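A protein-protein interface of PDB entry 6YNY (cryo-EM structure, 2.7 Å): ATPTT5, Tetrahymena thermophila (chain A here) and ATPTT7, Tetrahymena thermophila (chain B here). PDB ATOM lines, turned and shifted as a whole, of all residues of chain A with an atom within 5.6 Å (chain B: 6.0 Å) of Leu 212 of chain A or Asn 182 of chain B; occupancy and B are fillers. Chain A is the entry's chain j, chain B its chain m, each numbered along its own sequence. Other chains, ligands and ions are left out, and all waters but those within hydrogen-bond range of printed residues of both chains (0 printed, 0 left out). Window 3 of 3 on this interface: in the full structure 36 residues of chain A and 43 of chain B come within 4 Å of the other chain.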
ATOM      1  N   HIS A 206      11.101  19.552  17.475  1.00  0.00           N
ATOM      2  CA  HIS A 206      10.031  18.702  16.974  1.00  0.00           C
ATOM      3  C   HIS A 206      10.540  17.423  16.333  1.00  0.00           C
ATOM      4  O   HIS A 206       9.731  16.546  16.015  1.00  0.00           O
ATOM      5  CB  HIS A 206       9.178  19.475  15.975  1.00  0.00           C
ATOM      6  CG  HIS A 206       8.388  20.582  16.595  1.00  0.00           C
ATOM      7  ND1 HIS A 206       8.968  21.741  17.059  1.00  0.00           N
ATOM      8  CD2 HIS A 206       7.063  20.700  16.838  1.00  0.00           C
ATOM      9  CE1 HIS A 206       8.034  22.530  17.556  1.00  0.00           C
ATOM     10  NE2 HIS A 206       6.868  21.922  17.434  1.00  0.00           N
ATOM     11  N   GLY A 207      11.851  17.296  16.134  1.00  0.00           N
ATOM     12  CA  GLY A 207      12.440  16.082  15.618  1.00  0.00           C
ATOM     13  C   GLY A 207      13.218  15.285  16.636  1.00  0.00           C
ATOM     14  O   GLY A 207      13.950  14.364  16.250  1.00  0.00           O
ATOM     15  N   THR A 208      13.088  15.594  17.921  1.00  0.00           N
ATOM     16  CA  THR A 208      13.852  14.923  18.958  1.00  0.00           C
ATOM     17  C   THR A 208      13.070  13.726  19.495  1.00  0.00           C
ATOM     18  O   THR A 208      12.035  13.331  18.955  1.00  0.00           O
ATOM     19  CB  THR A 208      14.210  15.908  20.065  1.00  0.00           C
ATOM     20  OG1 THR A 208      13.018  16.520  20.571  1.00  0.00           O
ATOM     21  CG2 THR A 208      15.139  16.974  19.533  1.00  0.00           C
ATOM     22  N   ARG A 209      13.567  13.142  20.584  1.00  0.00           N
ATOM     23  CA  ARG A 209      12.989  11.913  21.111  1.00  0.00           C
ATOM     24  C   ARG A 209      11.619  12.143  21.734  1.00  0.00           C
ATOM     25  O   ARG A 209      10.790  11.229  21.752  1.00  0.00           O
ATOM     26  CB  ARG A 209      13.950  11.303  22.130  1.00  0.00           C
ATOM     27  CG  ARG A 209      13.377  10.178  22.945  1.00  0.00           C
ATOM     28  CD  ARG A 209      14.470   9.435  23.671  1.00  0.00           C
ATOM     29  NE  ARG A 209      15.269  10.304  24.526  1.00  0.00           N
ATOM     30  CZ  ARG A 209      15.021  10.536  25.809  1.00  0.00           C
ATOM     31  NH1 ARG A 209      13.989   9.967  26.412  1.00  0.00           N
ATOM     32  NH2 ARG A 209      15.814  11.342  26.494  1.00  0.00           N
ATOM     33  N   GLN A 210      11.365  13.346  22.247  1.00  0.00           N
ATOM     34  CA  GLN A 210      10.093  13.607  22.908  1.00  0.00           C
ATOM     35  C   GLN A 210       8.944  13.706  21.913  1.00  0.00           C
ATOM     36  O   GLN A 210       7.808  13.355  22.248  1.00  0.00           O
ATOM     37  CB  GLN A 210      10.189  14.885  23.735  1.00  0.00           C
ATOM     38  CG  GLN A 210      11.294  14.863  24.776  1.00  0.00           C
ATOM     39  CD  GLN A 210      11.109  13.760  25.797  1.00  0.00           C
ATOM     40  OE1 GLN A 210      10.030  13.182  25.914  1.00  0.00           O
ATOM     41  NE2 GLN A 210      12.165  13.460  26.540  1.00  0.00           N
ATOM     42  N   HIS A 211       9.213  14.174  20.699  1.00  0.00           N
ATOM     43  CA  HIS A 211       8.188  14.358  19.681  1.00  0.00           C
ATOM     44  C   HIS A 211       8.256  13.337  18.559  1.00  0.00           C
ATOM     45  O   HIS A 211       7.213  12.890  18.078  1.00  0.00           O
ATOM     46  CB  HIS A 211       8.294  15.761  19.083  1.00  0.00           C
ATOM     47  CG  HIS A 211       8.135  16.855  20.090  1.00  0.00           C
ATOM     48  ND1 HIS A 211       9.115  17.170  21.006  1.00  0.00           N
ATOM     49  CD2 HIS A 211       7.108  17.703  20.331  1.00  0.00           C
ATOM     50  CE1 HIS A 211       8.701  18.167  21.764  1.00  0.00           C
ATOM     51  NE2 HIS A 211       7.486  18.510  21.375  1.00  0.00           N
ATOM     52  N   LEU A 212       9.452  12.962  18.125  1.00  0.00           N
ATOM     53  CA  LEU A 212       9.641  11.986  17.061  1.00  0.00           C
ATOM     54  C   LEU A 212      10.232  10.723  17.666  1.00  0.00           C
ATOM     55  O   LEU A 212      11.362  10.738  18.164  1.00  0.00           O
ATOM     56  CB  LEU A 212      10.553  12.541  15.969  1.00  0.00           C
ATOM     57  CG  LEU A 212      10.727  11.668  14.729  1.00  0.00           C
ATOM     58  CD1 LEU A 212       9.417  11.503  14.001  1.00  0.00           C
ATOM     59  CD2 LEU A 212      11.763  12.264  13.812  1.00  0.00           C
ATOM     60  N   ARG A 213       9.474   9.640  17.620  1.00  0.00           N
ATOM     61  CA  ARG A 213       9.910   8.404  18.248  1.00  0.00           C
ATOM     62  C   ARG A 213      11.087   7.815  17.477  1.00  0.00           C
ATOM     63  O   ARG A 213      11.020   7.702  16.249  1.00  0.00           O
ATOM     64  CB  ARG A 213       8.768   7.401  18.297  1.00  0.00           C
ATOM     65  CG  ARG A 213       8.821   6.477  19.487  1.00  0.00           C
ATOM     66  CD  ARG A 213       7.872   5.319  19.322  1.00  0.00           C
ATOM     67  NE  ARG A 213       8.506   4.204  18.629  1.00  0.00           N
ATOM     68  CZ  ARG A 213       9.102   3.185  19.238  1.00  0.00           C
ATOM     69  NH1 ARG A 213       9.152   3.120  20.560  1.00  0.00           N
ATOM     70  NH2 ARG A 213       9.651   2.220  18.521  1.00  0.00           N
ATOM     71  N   PRO A 214      12.172   7.433  18.147  1.00  0.00           N
ATOM     72  CA  PRO A 214      13.270   6.766  17.443  1.00  0.00           C
ATOM     73  C   PRO A 214      12.836   5.426  16.873  1.00  0.00           C
ATOM     74  O   PRO A 214      11.756   4.905  17.159  1.00  0.00           O
ATOM     75  CB  PRO A 214      14.339   6.596  18.523  1.00  0.00           C
ATOM     76  CG  PRO A 214      14.002   7.591  19.556  1.00  0.00           C
ATOM     77  CD  PRO A 214      12.523   7.713  19.548  1.00  0.00           C
ATOM     78  N   ASP A 215      13.711   4.862  16.049  1.00  0.00           N
ATOM     79  CA  ASP A 215      13.459   3.574  15.407  1.00  0.00           C
ATOM     80  C   ASP A 215      13.950   2.419  16.274  1.00  0.00           C
ATOM     81  O   ASP A 215      14.724   1.567  15.840  1.00  0.00           O
ATOM     82  CB  ASP A 215      14.113   3.548  14.032  1.00  0.00           C
ATOM     83  CG  ASP A 215      13.684   2.357  13.207  1.00  0.00           C
ATOM     84  OD1 ASP A 215      12.877   1.546  13.703  1.00  0.00           O
ATOM     85  OD2 ASP A 215      14.152   2.232  12.057  1.00  0.00           O
ATOM     86  N   GLN B  16      18.801  10.499  21.433  1.00  0.00           N
ATOM     87  CA  GLN B  16      18.394   9.117  21.252  1.00  0.00           C
ATOM     88  C   GLN B  16      19.641   8.277  21.010  1.00  0.00           C
ATOM     89  O   GLN B  16      20.771   8.750  21.156  1.00  0.00           O
ATOM     90  CB  GLN B  16      17.384   9.001  20.103  1.00  0.00           C
ATOM     91  CG  GLN B  16      17.965   9.263  18.735  1.00  0.00           C
ATOM     92  CD  GLN B  16      16.902   9.490  17.686  1.00  0.00           C
ATOM     93  OE1 GLN B  16      16.770   8.717  16.740  1.00  0.00           O
ATOM     94  NE2 GLN B  16      16.142  10.566  17.844  1.00  0.00           N
ATOM     95  N   ARG B  28      22.194   5.413   8.200  1.00  0.00           N
ATOM     96  CA  ARG B  28      21.950   6.672   8.888  1.00  0.00           C
ATOM     97  C   ARG B  28      23.165   7.586   8.828  1.00  0.00           C
ATOM     98  O   ARG B  28      23.017   8.813   8.859  1.00  0.00           O
ATOM     99  CB  ARG B  28      21.558   6.387  10.332  1.00  0.00           C
ATOM    100  CG  ARG B  28      21.014   7.567  11.091  1.00  0.00           C
ATOM    101  CD  ARG B  28      20.673   7.158  12.499  1.00  0.00           C
ATOM    102  NE  ARG B  28      20.031   8.223  13.260  1.00  0.00           N
ATOM    103  CZ  ARG B  28      18.725   8.467  13.251  1.00  0.00           C
ATOM    104  NH1 ARG B  28      17.908   7.732  12.515  1.00  0.00           N
ATOM    105  NH2 ARG B  28      18.234   9.452  13.982  1.00  0.00           N
ATOM    106  N   ARG B 179      14.706  17.201  12.058  1.00  0.00           N
ATOM    107  CA  ARG B 179      14.561  15.861  11.517  1.00  0.00           C
ATOM    108  C   ARG B 179      13.085  15.565  11.290  1.00  0.00           C
ATOM    109  O   ARG B 179      12.251  15.796  12.170  1.00  0.00           O
ATOM    110  CB  ARG B 179      15.175  14.831  12.461  1.00  0.00           C
ATOM    111  CG  ARG B 179      15.016  13.405  11.993  1.00  0.00           C
ATOM    112  CD  ARG B 179      15.754  12.430  12.880  1.00  0.00           C
ATOM    113  NE  ARG B 179      17.179  12.373  12.584  1.00  0.00           N
ATOM    114  CZ  ARG B 179      17.704  11.672  11.586  1.00  0.00           C
ATOM    115  NH1 ARG B 179      16.925  10.971  10.777  1.00  0.00           N
ATOM    116  NH2 ARG B 179      19.011  11.675  11.390  1.00  0.00           N
ATOM    117  N   GLN B 180      12.772  15.054  10.103  1.00  0.00           N
ATOM    118  CA  GLN B 180      11.398  14.802   9.696  1.00  0.00           C
ATOM    119  C   GLN B 180      11.005  13.338   9.789  1.00  0.00           C
ATOM    120  O   GLN B 180       9.809  13.037   9.852  1.00  0.00           O
ATOM    121  CB  GLN B 180      11.190  15.289   8.257  1.00  0.00           C
ATOM    122  CG  GLN B 180       9.773  15.201   7.750  1.00  0.00           C
ATOM    123  CD  GLN B 180       9.649  15.694   6.328  1.00  0.00           C
ATOM    124  OE1 GLN B 180      10.599  16.229   5.761  1.00  0.00           O
ATOM    125  NE2 GLN B 180       8.475  15.510   5.737  1.00  0.00           N
ATOM    126  N   ALA B 181      11.973  12.427   9.803  1.00  0.00           N
ATOM    127  CA  ALA B 181      11.688  11.004   9.803  1.00  0.00           C
ATOM    128  C   ALA B 181      12.849  10.262  10.446  1.00  0.00           C
ATOM    129  O   ALA B 181      13.848  10.858  10.854  1.00  0.00           O
ATOM    130  CB  ALA B 181      11.437  10.504   8.381  1.00  0.00           C
ATOM    131  N   ASN B 182      12.701   8.943  10.535  1.00  0.00           N
ATOM    132  CA  ASN B 182      13.732   8.052  11.051  1.00  0.00           C
ATOM    133  C   ASN B 182      13.846   6.818  10.171  1.00  0.00           C
ATOM    134  O   ASN B 182      14.061   5.703  10.653  1.00  0.00           O
ATOM    135  CB  ASN B 182      13.456   7.663  12.500  1.00  0.00           C
ATOM    136  CG  ASN B 182      13.971   8.685  13.482  1.00  0.00           C
ATOM    137  OD1 ASN B 182      15.046   9.250  13.297  1.00  0.00           O
ATOM    138  ND2 ASN B 182      13.211   8.928  14.534  1.00  0.00           N
ATOM    139  N   ASN B 183      13.695   7.004   8.864  1.00  0.00           N
ATOM    140  CA  ASN B 183      13.865   5.920   7.909  1.00  0.00           C
ATOM    141  C   ASN B 183      15.317   5.716   7.508  1.00  0.00           C
ATOM    142  O   ASN B 183      15.600   4.829   6.697  1.00  0.00           O
ATOM    143  CB  ASN B 183      13.022   6.185   6.662  1.00  0.00           C
ATOM    144  CG  ASN B 183      11.541   6.170   6.951  1.00  0.00           C
ATOM    145  OD1 ASN B 183      11.050   5.323   7.693  1.00  0.00           O
ATOM    146  ND2 ASN B 183      10.819   7.116   6.371  1.00  0.00           N
ATOM    147  N   HIS B 184      16.234   6.516   8.050  1.00  0.00           N
ATOM    148  CA  HIS B 184      17.662   6.378   7.782  1.00  0.00           C
ATOM    149  C   HIS B 184      17.991   6.712   6.331  1.00  0.00           C
ATOM    150  O   HIS B 184      18.832   6.068   5.706  1.00  0.00           O
ATOM    151  CB  HIS B 184      18.151   4.977   8.142  1.00  0.00           C
ATOM    152  CG  HIS B 184      17.700   4.514   9.488  1.00  0.00           C
ATOM    153  ND1 HIS B 184      17.929   5.238  10.637  1.00  0.00           N
ATOM    154  CD2 HIS B 184      17.029   3.404   9.869  1.00  0.00           C
ATOM    155  CE1 HIS B 184      17.417   4.592  11.669  1.00  0.00           C
ATOM    156  NE2 HIS B 184      16.867   3.476  11.231  1.00  0.00           N
ATOM    157  N   LYS B 185      17.319   7.723   5.794  1.00  0.00           N
ATOM    158  CA  LYS B 185      17.544   8.186   4.438  1.00  0.00           C
ATOM    159  C   LYS B 185      17.695   9.700   4.447  1.00  0.00           C
ATOM    160  O   LYS B 185      17.372  10.374   5.428  1.00  0.00           O
ATOM    161  CB  LYS B 185      16.396   7.771   3.515  1.00  0.00           C
ATOM    162  CG  LYS B 185      16.145   6.282   3.478  1.00  0.00           C
ATOM    163  CD  LYS B 185      14.906   5.959   2.678  1.00  0.00           C
ATOM    164  CE  LYS B 185      14.602   4.478   2.707  1.00  0.00           C
ATOM    165  NZ  LYS B 185      13.311   4.166   2.035  1.00  0.00           N
ATOM    166  N   ASP B 188      14.929  12.165   5.468  1.00  0.00           N
ATOM    167  CA  ASP B 188      14.627  12.518   6.848  1.00  0.00           C
ATOM    168  C   ASP B 188      14.809  14.005   7.106  1.00  0.00           C
ATOM    169  O   ASP B 188      14.235  14.533   8.063  1.00  0.00           O
ATOM    170  CB  ASP B 188      15.510  11.708   7.793  1.00  0.00           C
ATOM    171  CG  ASP B 188      15.300  10.216   7.645  1.00  0.00           C
ATOM    172  OD1 ASP B 188      14.480   9.811   6.796  1.00  0.00           O
ATOM    173  OD2 ASP B 188      15.955   9.448   8.379  1.00  0.00           O
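The side-chain carboxylate (OD2) of Asp 215 of chain A sits at hydrogen-bond distance from a ring nitrogen (NE2) of His 184 of chain B, at 3.1 Å. O of Arg 213 of chain A is in hydrogen-bond range of ND2 of Asn 182 of chain B, at 3.0 Å.
N of His 184 of chain B sits at hydrogen-bond distance from OD2 of Asp 188 of chain B (3.0 Å). NH1 of Arg 179 of chain B lies close to O of Ala 181 of chain B. OD2 of Asp 188 of chain B is in salt-bridge range of NH1 of Arg 179 of chain B (3.0 Å). NH1 of Arg 28 of chain B sits at hydrogen-bond distance from ND1 of His 184 of chain B, 3.1 Å away. The side-chain amide oxygen (OE1) of Gln 16 of chain B sits at hydrogen-bond distance from the guanidinium group (NH2) of Arg 28 of chain B (3.2 Å). NH2 of Arg 28 of chain B is in hydrogen-bond range of OD1 of Asn 182 of chain B (3.3 Å).
Gly 207 of chain A touches Arg 179 of chain B (CA to O, 3.5 Å). Leu 212 of chain A touches Arg 179 of chain B (CD2 to CG, 3.9 Å). Ala 181 of chain B touches Leu 212 of chain A. ND2 of Asn 182 of chain B touches CG of Leu 212 of chain A, 3.7 Å away. CB of Pro 214 of chain A touches OE1 of Gln 16 of chain B (3.7 Å). Pro 214 of chain A touches Asn 182 of chain B. OD2 of Asp 215 of chain A touches O of Asn 182 of chain B, 3.7 Å away.
Of the printed residues of chain B, Gly 207 of chain A touches Arg 179. Printed residues of chain B within 4 Å of Arg 213 of chain A: Asn 182 (3.0 Å). Printed residues of chain B within 4 Å of Asp 215 of chain A: Asn 182 (3.7 Å) and His 184 (3.1 Å). Asn 182 of chain B touches just these residues of chain A: Leu 212, Arg 213, Pro 214 and Asp 215. Asn 183 of chain B touches none of the printed residues of chain A. The nearest residue of chain B that does not touch Leu 212 of chain A is Gln 180 of chain B (4.2 Å).
Hydrophobic or aromatic side chains of chain A that line the printed part of chain B: Leu 212 and Pro 214. Among the printed residues, no Asp or Glu carboxylate lies within 4 Å of a Lys or Arg side-chain nitrogen of the other chain.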
